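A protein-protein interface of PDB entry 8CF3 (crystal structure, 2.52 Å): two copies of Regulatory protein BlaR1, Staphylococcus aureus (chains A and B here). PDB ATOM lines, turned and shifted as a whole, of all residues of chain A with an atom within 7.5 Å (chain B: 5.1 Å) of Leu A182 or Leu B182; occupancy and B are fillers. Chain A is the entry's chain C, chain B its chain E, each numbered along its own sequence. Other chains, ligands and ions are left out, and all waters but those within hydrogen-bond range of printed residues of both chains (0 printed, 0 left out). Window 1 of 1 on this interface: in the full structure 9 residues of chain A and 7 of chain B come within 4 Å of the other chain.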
ATOM      1  N   ASN A  99      14.115   1.062  -6.726  1.00  0.00           N
ATOM      2  CA  ASN A  99      14.630   1.095  -8.084  1.00  0.00           C
ATOM      3  C   ASN A  99      14.243   2.406  -8.764  1.00  0.00           C
ATOM      4  O   ASN A  99      15.105   3.068  -9.332  1.00  0.00           O
ATOM      5  CB  ASN A  99      14.155  -0.120  -8.882  1.00  0.00           C
ATOM      6  CG  ASN A  99      14.724  -1.429  -8.368  1.00  0.00           C
ATOM      7  OD1 ASN A  99      15.573  -1.449  -7.478  1.00  0.00           O
ATOM      8  ND2 ASN A  99      14.249  -2.534  -8.918  1.00  0.00           N
ATOM      9  N   MET A 102      15.886   5.413  -6.981  1.00  0.00           N
ATOM     10  CA  MET A 102      17.318   5.506  -7.233  1.00  0.00           C
ATOM     11  C   MET A 102      17.565   5.952  -8.673  1.00  0.00           C
ATOM     12  O   MET A 102      18.387   6.834  -8.922  1.00  0.00           O
ATOM     13  CB  MET A 102      17.998   4.151  -6.994  1.00  0.00           C
ATOM     14  CG  MET A 102      19.527   4.216  -6.923  1.00  0.00           C
ATOM     15  SD  MET A 102      20.132   5.183  -5.506  1.00  0.00           S
ATOM     16  CE  MET A 102      19.837   4.021  -4.174  1.00  0.00           C
ATOM     17  N   GLN A 103      16.818   5.352  -9.603  1.00  0.00           N
ATOM     18  CA  GLN A 103      16.985   5.571 -11.033  1.00  0.00           C
ATOM     19  C   GLN A 103      16.665   7.019 -11.405  1.00  0.00           C
ATOM     20  O   GLN A 103      17.271   7.568 -12.323  1.00  0.00           O
ATOM     21  CB  GLN A 103      16.088   4.584 -11.785  1.00  0.00           C
ATOM     22  CG  GLN A 103      16.012   4.806 -13.289  1.00  0.00           C
ATOM     23  CD  GLN A 103      14.877   4.035 -13.924  1.00  0.00           C
ATOM     24  OE1 GLN A 103      14.220   3.199 -13.301  1.00  0.00           O
ATOM     25  NE2 GLN A 103      14.635   4.311 -15.193  1.00  0.00           N
ATOM     26  N   GLN A 176      20.090  -6.080  -3.226  1.00  0.00           N
ATOM     27  CA  GLN A 176      18.958  -5.209  -3.486  1.00  0.00           C
ATOM     28  C   GLN A 176      19.459  -3.809  -3.833  1.00  0.00           C
ATOM     29  O   GLN A 176      18.954  -3.190  -4.765  1.00  0.00           O
ATOM     30  CB  GLN A 176      17.991  -5.168  -2.305  1.00  0.00           C
ATOM     31  CG  GLN A 176      16.672  -4.502  -2.675  1.00  0.00           C
ATOM     32  CD  GLN A 176      15.604  -4.660  -1.625  1.00  0.00           C
ATOM     33  OE1 GLN A 176      15.777  -5.360  -0.630  1.00  0.00           O
ATOM     34  NE2 GLN A 176      14.481  -3.999  -1.846  1.00  0.00           N
ATOM     35  N   LEU A 177      20.461  -3.319  -3.093  1.00  0.00           N
ATOM     36  CA  LEU A 177      21.077  -2.043  -3.415  1.00  0.00           C
ATOM     37  C   LEU A 177      21.654  -2.108  -4.824  1.00  0.00           C
ATOM     38  O   LEU A 177      21.455  -1.201  -5.629  1.00  0.00           O
ATOM     39  CB  LEU A 177      22.176  -1.721  -2.396  1.00  0.00           C
ATOM     40  CG  LEU A 177      23.074  -0.538  -2.763  1.00  0.00           C
ATOM     41  CD1 LEU A 177      22.267   0.743  -2.923  1.00  0.00           C
ATOM     42  CD2 LEU A 177      24.172  -0.338  -1.730  1.00  0.00           C
ATOM     43  N   SER A 178      22.372  -3.199  -5.104  1.00  0.00           N
ATOM     44  CA  SER A 178      23.050  -3.373  -6.376  1.00  0.00           C
ATOM     45  C   SER A 178      22.048  -3.358  -7.533  1.00  0.00           C
ATOM     46  O   SER A 178      22.309  -2.738  -8.558  1.00  0.00           O
ATOM     47  CB  SER A 178      23.876  -4.628  -6.358  1.00  0.00           C
ATOM     48  OG  SER A 178      24.611  -4.749  -7.555  1.00  0.00           O
ATOM     49  N   SER A 179      20.904  -4.031  -7.352  1.00  0.00           N
ATOM     50  CA  SER A 179      19.814  -4.020  -8.320  1.00  0.00           C
ATOM     51  C   SER A 179      19.359  -2.596  -8.640  1.00  0.00           C
ATOM     52  O   SER A 179      19.111  -2.266  -9.798  1.00  0.00           O
ATOM     53  CB  SER A 179      18.651  -4.844  -7.835  1.00  0.00           C
ATOM     54  OG  SER A 179      18.936  -6.230  -7.958  1.00  0.00           O
ATOM     55  N   SER A 180      19.252  -1.756  -7.609  1.00  0.00           N
ATOM     56  CA  SER A 180      18.753  -0.401  -7.785  1.00  0.00           C
ATOM     57  C   SER A 180      19.759   0.479  -8.527  1.00  0.00           C
ATOM     58  O   SER A 180      19.413   1.575  -8.956  1.00  0.00           O
ATOM     59  CB  SER A 180      18.387   0.214  -6.461  1.00  0.00           C
ATOM     60  OG  SER A 180      19.550   0.530  -5.715  1.00  0.00           O
ATOM     61  N   LEU A 181      21.002   0.004  -8.670  1.00  0.00           N
ATOM     62  CA  LEU A 181      22.074   0.808  -9.233  1.00  0.00           C
ATOM     63  C   LEU A 181      22.456   0.355 -10.639  1.00  0.00           C
ATOM     64  O   LEU A 181      23.221   1.048 -11.298  1.00  0.00           O
ATOM     65  CB  LEU A 181      23.277   0.716  -8.296  1.00  0.00           C
ATOM     66  CG  LEU A 181      23.181   1.513  -6.998  1.00  0.00           C
ATOM     67  CD1 LEU A 181      24.392   1.226  -6.126  1.00  0.00           C
ATOM     68  CD2 LEU A 181      23.064   3.003  -7.280  1.00  0.00           C
ATOM     69  N   LEU A 182      21.925  -0.785 -11.103  1.00  0.00           N
ATOM     70  CA  LEU A 182      22.257  -1.303 -12.421  1.00  0.00           C
ATOM     71  C   LEU A 182      21.739  -0.354 -13.497  1.00  0.00           C
ATOM     72  O   LEU A 182      20.569   0.018 -13.494  1.00  0.00           O
ATOM     73  CB  LEU A 182      21.666  -2.709 -12.592  1.00  0.00           C
ATOM     74  CG  LEU A 182      21.946  -3.381 -13.937  1.00  0.00           C
ATOM     75  CD1 LEU A 182      23.424  -3.695 -14.116  1.00  0.00           C
ATOM     76  CD2 LEU A 182      21.123  -4.651 -14.088  1.00  0.00           C
ATOM     77  N   ILE A 183      22.628   0.003 -14.429  1.00  0.00           N
ATOM     78  CA  ILE A 183      22.337   0.971 -15.473  1.00  0.00           C
ATOM     79  C   ILE A 183      22.366   0.285 -16.837  1.00  0.00           C
ATOM     80  O   ILE A 183      21.476   0.504 -17.657  1.00  0.00           O
ATOM     81  CB  ILE A 183      23.345   2.136 -15.404  1.00  0.00           C
ATOM     82  CG1 ILE A 183      23.156   2.952 -14.125  1.00  0.00           C
ATOM     83  CG2 ILE A 183      23.266   3.012 -16.651  1.00  0.00           C
ATOM     84  CD1 ILE A 183      24.316   3.857 -13.817  1.00  0.00           C
ATOM     85  N   LYS A 184      23.431  -0.492 -17.084  1.00  0.00           N
ATOM     86  CA  LYS A 184      23.650  -1.123 -18.373  1.00  0.00           C
ATOM     87  C   LYS A 184      24.181  -2.534 -18.146  1.00  0.00           C
ATOM     88  O   LYS A 184      24.901  -2.783 -17.182  1.00  0.00           O
ATOM     89  CB  LYS A 184      24.616  -0.285 -19.218  1.00  0.00           C
ATOM     90  CG  LYS A 184      24.637  -0.648 -20.694  1.00  0.00           C
ATOM     91  CD  LYS A 184      25.202   0.409 -21.622  1.00  0.00           C
ATOM     92  CE  LYS A 184      25.084  -0.022 -23.074  1.00  0.00           C
ATOM     93  NZ  LYS A 184      25.888   0.830 -23.985  1.00  0.00           N
ATOM     94  N   LYS A 185      23.781  -3.452 -19.036  1.00  0.00           N
ATOM     95  CA  LYS A 185      24.250  -4.829 -19.013  1.00  0.00           C
ATOM     96  C   LYS A 185      24.271  -5.382 -20.437  1.00  0.00           C
ATOM     97  O   LYS A 185      23.348  -5.144 -21.210  1.00  0.00           O
ATOM     98  CB  LYS A 185      23.374  -5.677 -18.086  1.00  0.00           C
ATOM     99  CG  LYS A 185      23.594  -7.181 -18.174  1.00  0.00           C
ATOM    100  CD  LYS A 185      22.903  -7.952 -17.077  1.00  0.00           C
ATOM    101  CE  LYS A 185      23.027  -9.452 -17.238  1.00  0.00           C
ATOM    102  NZ  LYS A 185      24.433  -9.906 -17.132  1.00  0.00           N
ATOM    103  N   ASN A 186      25.350  -6.101 -20.765  1.00  0.00           N
ATOM    104  CA  ASN A 186      25.488  -6.808 -22.028  1.00  0.00           C
ATOM    105  C   ASN A 186      26.389  -8.023 -21.797  1.00  0.00           C
ATOM    106  O   ASN A 186      26.706  -8.343 -20.654  1.00  0.00           O
ATOM    107  CB  ASN A 186      25.969  -5.875 -23.146  1.00  0.00           C
ATOM    108  CG  ASN A 186      27.405  -5.415 -23.003  1.00  0.00           C
ATOM    109  OD1 ASN A 186      28.084  -5.728 -22.025  1.00  0.00           O
ATOM    110  ND2 ASN A 186      27.883  -4.655 -23.976  1.00  0.00           N
ATOM    111  N   TYR A 189      29.765  -6.712 -19.883  1.00  0.00           N
ATOM    112  CA  TYR A 189      29.841  -6.042 -18.594  1.00  0.00           C
ATOM    113  C   TYR A 189      28.466  -5.712 -18.016  1.00  0.00           C
ATOM    114  O   TYR A 189      27.482  -5.573 -18.744  1.00  0.00           O
ATOM    115  CB  TYR A 189      30.668  -4.759 -18.714  1.00  0.00           C
ATOM    116  CG  TYR A 189      30.067  -3.683 -19.583  1.00  0.00           C
ATOM    117  CD1 TYR A 189      29.112  -2.805 -19.093  1.00  0.00           C
ATOM    118  CD2 TYR A 189      30.457  -3.542 -20.904  1.00  0.00           C
ATOM    119  CE1 TYR A 189      28.564  -1.812 -19.892  1.00  0.00           C
ATOM    120  CE2 TYR A 189      29.922  -2.553 -21.716  1.00  0.00           C
ATOM    121  CZ  TYR A 189      28.970  -1.688 -21.210  1.00  0.00           C
ATOM    122  OH  TYR A 189      28.431  -0.716 -22.017  1.00  0.00           O
ATOM    123  N   GLU A 190      28.448  -5.589 -16.680  1.00  0.00           N
ATOM    124  CA  GLU A 190      27.381  -4.943 -15.933  1.00  0.00           C
ATOM    125  C   GLU A 190      27.909  -3.626 -15.368  1.00  0.00           C
ATOM    126  O   GLU A 190      28.906  -3.620 -14.648  1.00  0.00           O
ATOM    127  CB  GLU A 190      26.916  -5.833 -14.780  1.00  0.00           C
ATOM    128  CG  GLU A 190      26.222  -7.103 -15.227  1.00  0.00           C
ATOM    129  CD  GLU A 190      25.794  -8.027 -14.097  1.00  0.00           C
ATOM    130  OE1 GLU A 190      26.216  -7.788 -12.947  1.00  0.00           O
ATOM    131  OE2 GLU A 190      25.040  -8.993 -14.373  1.00  0.00           O
ATOM    132  N   LEU A 191      27.225  -2.520 -15.680  1.00  0.00           N
ATOM    133  CA  LEU A 191      27.612  -1.204 -15.200  1.00  0.00           C
ATOM    134  C   LEU A 191      26.616  -0.757 -14.136  1.00  0.00           C
ATOM    135  O   LEU A 191      25.418  -0.744 -14.385  1.00  0.00           O
ATOM    136  CB  LEU A 191      27.629  -0.230 -16.382  1.00  0.00           C
ATOM    137  CG  LEU A 191      27.913   1.231 -16.038  1.00  0.00           C
ATOM    138  CD1 LEU A 191      29.313   1.387 -15.475  1.00  0.00           C
ATOM    139  CD2 LEU A 191      27.726   2.116 -17.263  1.00  0.00           C
ATOM    140  N   TYR A 192      27.128  -0.392 -12.957  1.00  0.00           N
ATOM    141  CA  TYR A 192      26.304   0.138 -11.886  1.00  0.00           C
ATOM    142  C   TYR A 192      26.824   1.517 -11.502  1.00  0.00           C
ATOM    143  O   TYR A 192      28.019   1.775 -11.625  1.00  0.00           O
ATOM    144  CB  TYR A 192      26.338  -0.761 -10.649  1.00  0.00           C
ATOM    145  CG  TYR A 192      26.025  -2.215 -10.882  1.00  0.00           C
ATOM    146  CD1 TYR A 192      26.933  -3.053 -11.508  1.00  0.00           C
ATOM    147  CD2 TYR A 192      24.834  -2.766 -10.444  1.00  0.00           C
ATOM    148  CE1 TYR A 192      26.659  -4.397 -11.701  1.00  0.00           C
ATOM    149  CE2 TYR A 192      24.539  -4.106 -10.637  1.00  0.00           C
ATOM    150  CZ  TYR A 192      25.456  -4.925 -11.267  1.00  0.00           C
ATOM    151  OH  TYR A 192      25.163  -6.252 -11.446  1.00  0.00           O
ATOM    152  N   GLY A 193      25.936   2.388 -11.014  1.00  0.00           N
ATOM    153  CA  GLY A 193      26.364   3.708 -10.592  1.00  0.00           C
ATOM    154  C   GLY A 193      25.220   4.621 -10.164  1.00  0.00           C
ATOM    155  O   GLY A 193      24.044   4.270 -10.272  1.00  0.00           O
ATOM    156  N   TYR A 212      30.342   0.951 -10.090  1.00  0.00           N
ATOM    157  CA  TYR A 212      31.267  -0.142 -10.324  1.00  0.00           C
ATOM    158  C   TYR A 212      30.864  -0.932 -11.565  1.00  0.00           C
ATOM    159  O   TYR A 212      29.732  -0.837 -12.030  1.00  0.00           O
ATOM    160  CB  TYR A 212      31.363  -1.051  -9.097  1.00  0.00           C
ATOM    161  CG  TYR A 212      30.083  -1.711  -8.655  1.00  0.00           C
ATOM    162  CD1 TYR A 212      29.221  -1.092  -7.766  1.00  0.00           C
ATOM    163  CD2 TYR A 212      29.752  -2.977  -9.102  1.00  0.00           C
ATOM    164  CE1 TYR A 212      28.057  -1.715  -7.340  1.00  0.00           C
ATOM    165  CE2 TYR A 212      28.588  -3.609  -8.694  1.00  0.00           C
ATOM    166  CZ  TYR A 212      27.743  -2.979  -7.807  1.00  0.00           C
ATOM    167  OH  TYR A 212      26.600  -3.626  -7.416  1.00  0.00           O
ATOM    168  N   SER B 178      13.781 -13.149 -11.454  1.00  0.00           N
ATOM    169  CA  SER B 178      13.917 -12.181 -12.529  1.00  0.00           C
ATOM    170  C   SER B 178      15.371 -11.734 -12.677  1.00  0.00           C
ATOM    171  O   SER B 178      15.864 -11.620 -13.799  1.00  0.00           O
ATOM    172  CB  SER B 178      12.987 -11.014 -12.307  1.00  0.00           C
ATOM    173  OG  SER B 178      13.068 -10.096 -13.387  1.00  0.00           O
ATOM    174  N   SER B 179      16.049 -11.504 -11.540  1.00  0.00           N
ATOM    175  CA  SER B 179      17.469 -11.177 -11.516  1.00  0.00           C
ATOM    176  C   SER B 179      18.303 -12.237 -12.232  1.00  0.00           C
ATOM    177  O   SER B 179      19.217 -11.908 -12.985  1.00  0.00           O
ATOM    178  CB  SER B 179      17.963 -10.998 -10.104  1.00  0.00           C
ATOM    179  OG  SER B 179      17.505  -9.770  -9.560  1.00  0.00           O
ATOM    180  N   SER B 180      17.981 -13.513 -11.995  1.00  0.00           N
ATOM    181  CA  SER B 180      18.751 -14.612 -12.553  1.00  0.00           C
ATOM    182  C   SER B 180      18.544 -14.733 -14.062  1.00  0.00           C
ATOM    183  O   SER B 180      19.286 -15.461 -14.719  1.00  0.00           O
ATOM    184  CB  SER B 180      18.419 -15.909 -11.859  1.00  0.00           C
ATOM    185  OG  SER B 180      17.137 -16.369 -12.237  1.00  0.00           O
ATOM    186  N   LEU B 181      17.542 -14.031 -14.605  1.00  0.00           N
ATOM    187  CA  LEU B 181      17.169 -14.183 -16.001  1.00  0.00           C
ATOM    188  C   LEU B 181      17.582 -12.973 -16.840  1.00  0.00           C
ATOM    189  O   LEU B 181      17.478 -13.036 -18.061  1.00  0.00           O
ATOM    190  CB  LEU B 181      15.655 -14.398 -16.073  1.00  0.00           C
ATOM    191  CG  LEU B 181      15.154 -15.776 -15.639  1.00  0.00           C
ATOM    192  CD1 LEU B 181      13.632 -15.805 -15.628  1.00  0.00           C
ATOM    193  CD2 LEU B 181      15.690 -16.867 -16.555  1.00  0.00           C
ATOM    194  N   LEU B 182      18.042 -11.889 -16.203  1.00  0.00           N
ATOM    195  CA  LEU B 182      18.398 -10.675 -16.925  1.00  0.00           C
ATOM    196  C   LEU B 182      19.609 -10.934 -17.820  1.00  0.00           C
ATOM    197  O   LEU B 182      20.633 -11.438 -17.358  1.00  0.00           O
ATOM    198  CB  LEU B 182      18.682  -9.548 -15.925  1.00  0.00           C
ATOM    199  CG  LEU B 182      19.079  -8.200 -16.536  1.00  0.00           C
ATOM    200  CD1 LEU B 182      17.934  -7.581 -17.331  1.00  0.00           C
ATOM    201  CD2 LEU B 182      19.557  -7.232 -15.462  1.00  0.00           C
ATOM    202  N   ILE B 183      19.487 -10.554 -19.095  1.00  0.00           N
ATOM    203  CA  ILE B 183      20.497 -10.830 -20.106  1.00  0.00           C
ATOM    204  C   ILE B 183      21.102  -9.522 -20.612  1.00  0.00           C
ATOM    205  O   ILE B 183      22.317  -9.415 -20.747  1.00  0.00           O
ATOM    206  CB  ILE B 183      19.887 -11.653 -21.258  1.00  0.00           C
ATOM    207  CG1 ILE B 183      19.471 -13.050 -20.793  1.00  0.00           C
ATOM    208  CG2 ILE B 183      20.839 -11.722 -22.445  1.00  0.00           C
ATOM    209  CD1 ILE B 183      18.554 -13.767 -21.761  1.00  0.00           C
ATOM    210  N   LYS B 184      20.236  -8.555 -20.944  1.00  0.00           N
ATOM    211  CA  LYS B 184      20.667  -7.273 -21.478  1.00  0.00           C
ATOM    212  C   LYS B 184      19.844  -6.163 -20.831  1.00  0.00           C
ATOM    213  O   LYS B 184      18.671  -6.360 -20.526  1.00  0.00           O
ATOM    214  CB  LYS B 184      20.510  -7.232 -23.003  1.00  0.00           C
ATOM    215  CG  LYS B 184      21.535  -8.033 -23.788  1.00  0.00           C
ATOM    216  CD  LYS B 184      21.177  -8.264 -25.242  1.00  0.00           C
ATOM    217  CE  LYS B 184      22.172  -9.184 -25.924  1.00  0.00           C
ATOM    218  NZ  LYS B 184      21.724  -9.602 -27.273  1.00  0.00           N
ATOM    219  N   LYS B 185      20.489  -5.008 -20.609  1.00  0.00           N
ATOM    220  CA  LYS B 185      19.809  -3.812 -20.138  1.00  0.00           C
ATOM    221  C   LYS B 185      20.507  -2.582 -20.714  1.00  0.00           C
ATOM    222  O   LYS B 185      21.733  -2.512 -20.745  1.00  0.00           O
ATOM    223  CB  LYS B 185      19.771  -3.787 -18.608  1.00  0.00           C
ATOM    224  CG  LYS B 185      19.328  -2.470 -17.987  1.00  0.00           C
ATOM    225  CD  LYS B 185      19.097  -2.569 -16.494  1.00  0.00           C
ATOM    226  CE  LYS B 185      18.810  -1.235 -15.836  1.00  0.00           C
ATOM    227  NZ  LYS B 185      17.541  -0.641 -16.316  1.00  0.00           N
ATOM    228  N   GLU B 190      15.016  -3.678 -20.781  1.00  0.00           N
ATOM    229  CA  GLU B 190      15.575  -4.810 -20.059  1.00  0.00           C
ATOM    230  C   GLU B 190      15.093  -6.101 -20.723  1.00  0.00           C
ATOM    231  O   GLU B 190      13.891  -6.316 -20.847  1.00  0.00           O
ATOM    232  CB  GLU B 190      15.121  -4.808 -18.596  1.00  0.00           C
ATOM    233  CG  GLU B 190      15.574  -3.598 -17.798  1.00  0.00           C
ATOM    234  CD  GLU B 190      15.079  -3.558 -16.361  1.00  0.00           C
ATOM    235  OE1 GLU B 190      14.176  -4.344 -16.031  1.00  0.00           O
ATOM    236  OE2 GLU B 190      15.624  -2.753 -15.561  1.00  0.00           O
ATOM    237  N   LEU B 191      16.036  -6.958 -21.133  1.00  0.00           N
ATOM    238  CA  LEU B 191      15.717  -8.231 -21.759  1.00  0.00           C
ATOM    239  C   LEU B 191      15.992  -9.362 -20.775  1.00  0.00           C
ATOM    240  O   LEU B 191      17.089  -9.464 -20.255  1.00  0.00           O
ATOM    241  CB  LEU B 191      16.561  -8.386 -23.027  1.00  0.00           C
ATOM    242  CG  LEU B 191      16.406  -9.718 -23.766  1.00  0.00           C
ATOM    243  CD1 LEU B 191      15.002  -9.881 -24.303  1.00  0.00           C
ATOM    244  CD2 LEU B 191      17.407  -9.835 -24.903  1.00  0.00           C
ATOM    245  N   TYR B 192      14.994 -10.209 -20.529  1.00  0.00           N
ATOM    246  CA  TYR B 192      15.159 -11.386 -19.691  1.00  0.00           C
ATOM    247  C   TYR B 192      14.789 -12.625 -20.499  1.00  0.00           C
ATOM    248  O   TYR B 192      13.953 -12.542 -21.395  1.00  0.00           O
ATOM    249  CB  TYR B 192      14.260 -11.325 -18.456  1.00  0.00           C
ATOM    250  CG  TYR B 192      14.350 -10.064 -17.635  1.00  0.00           C
ATOM    251  CD1 TYR B 192      13.810  -8.868 -18.089  1.00  0.00           C
ATOM    252  CD2 TYR B 192      14.933 -10.075 -16.379  1.00  0.00           C
ATOM    253  CE1 TYR B 192      13.859  -7.715 -17.324  1.00  0.00           C
ATOM    254  CE2 TYR B 192      14.997  -8.930 -15.602  1.00  0.00           C
ATOM    255  CZ  TYR B 192      14.456  -7.745 -16.077  1.00  0.00           C
ATOM    256  OH  TYR B 192      14.512  -6.596 -15.324  1.00  0.00           O
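The backbone carbonyl oxygen of Lys B185 is in hydrogen-bond range of the backbone NH of Lys A185, 2.8 Å away.
Leu B182 touches its own counterpart, Leu A182.
Leu A182 touches Lys B185, and with the chains exchanged Lys A185 touches Leu B182.
Lys A184 touches Lys B185, and with the chains exchanged Lys A185 touches Lys B184.
Lys A185 touches its own counterpart, Lys B185.
Among the printed residues, pairs that only touch across the chains: Lys A185 with Leu B182, Leu A182 with Lys B185, Leu A182 with Leu B182, Lys A184 with Lys B185, Lys A185 with Lys B184, Lys A185 with Ile B183 and Ile A183 with Lys B185.
Leu A182 touches just these residues of chain B: Leu B182 and Lys B185.
Of the printed residues of chain B, Ile A183 touches Lys B185 (3.7 Å).
Of the printed residues of chain B, Lys A185 touches Leu B182 (3.1 Å), Ile B183 (3.6 Å), Lys B184 (3.4 Å) and Lys B185 (2.8 Å).
Of chain A, only Leu A182 (3.3 Å) and Lys A185 (3.1 Å) come within 4 Å of Leu B182.
Printed residues of chain A within 4 Å of Ile B183: Lys A185.
Of the printed residues of chain A, Lys B185 touches Leu A182, Ile A183, Lys A184 and Lys A185.
The backbone carbonyl oxygen of Leu A191 sits at hydrogen-bond distance from the backbone NH of Ile A183.
The backbone NH (N) of Leu A191 lies within hydrogen-bond range of the backbone carbonyl oxygen (O) of Lys A184 (2.8 Å).
NZ of Lys A185 lies within salt-bridge range of OE2 of Glu A190, at 3.0 Å.
The backbone NH (N) of Ile B183 lies within hydrogen-bond range of the backbone carbonyl oxygen (O) of Leu B191.
The backbone carbonyl oxygen (O) of Lys B184 is in hydrogen-bond range of the backbone NH (N) of Leu B191.
The side-chain amino group of Lys B185 is in salt-bridge range of the side-chain carboxylate of Glu B190 (3.0 Å).
Of the 20 printed residues of chain A, 4 touch a printed residue of chain B.
Of the 11 printed residues of chain B, 4 touch a printed residue of chain A.
Hydrophobic or aromatic side chains of chain B within 4 Å of the printed part of chain A: Leu B182.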
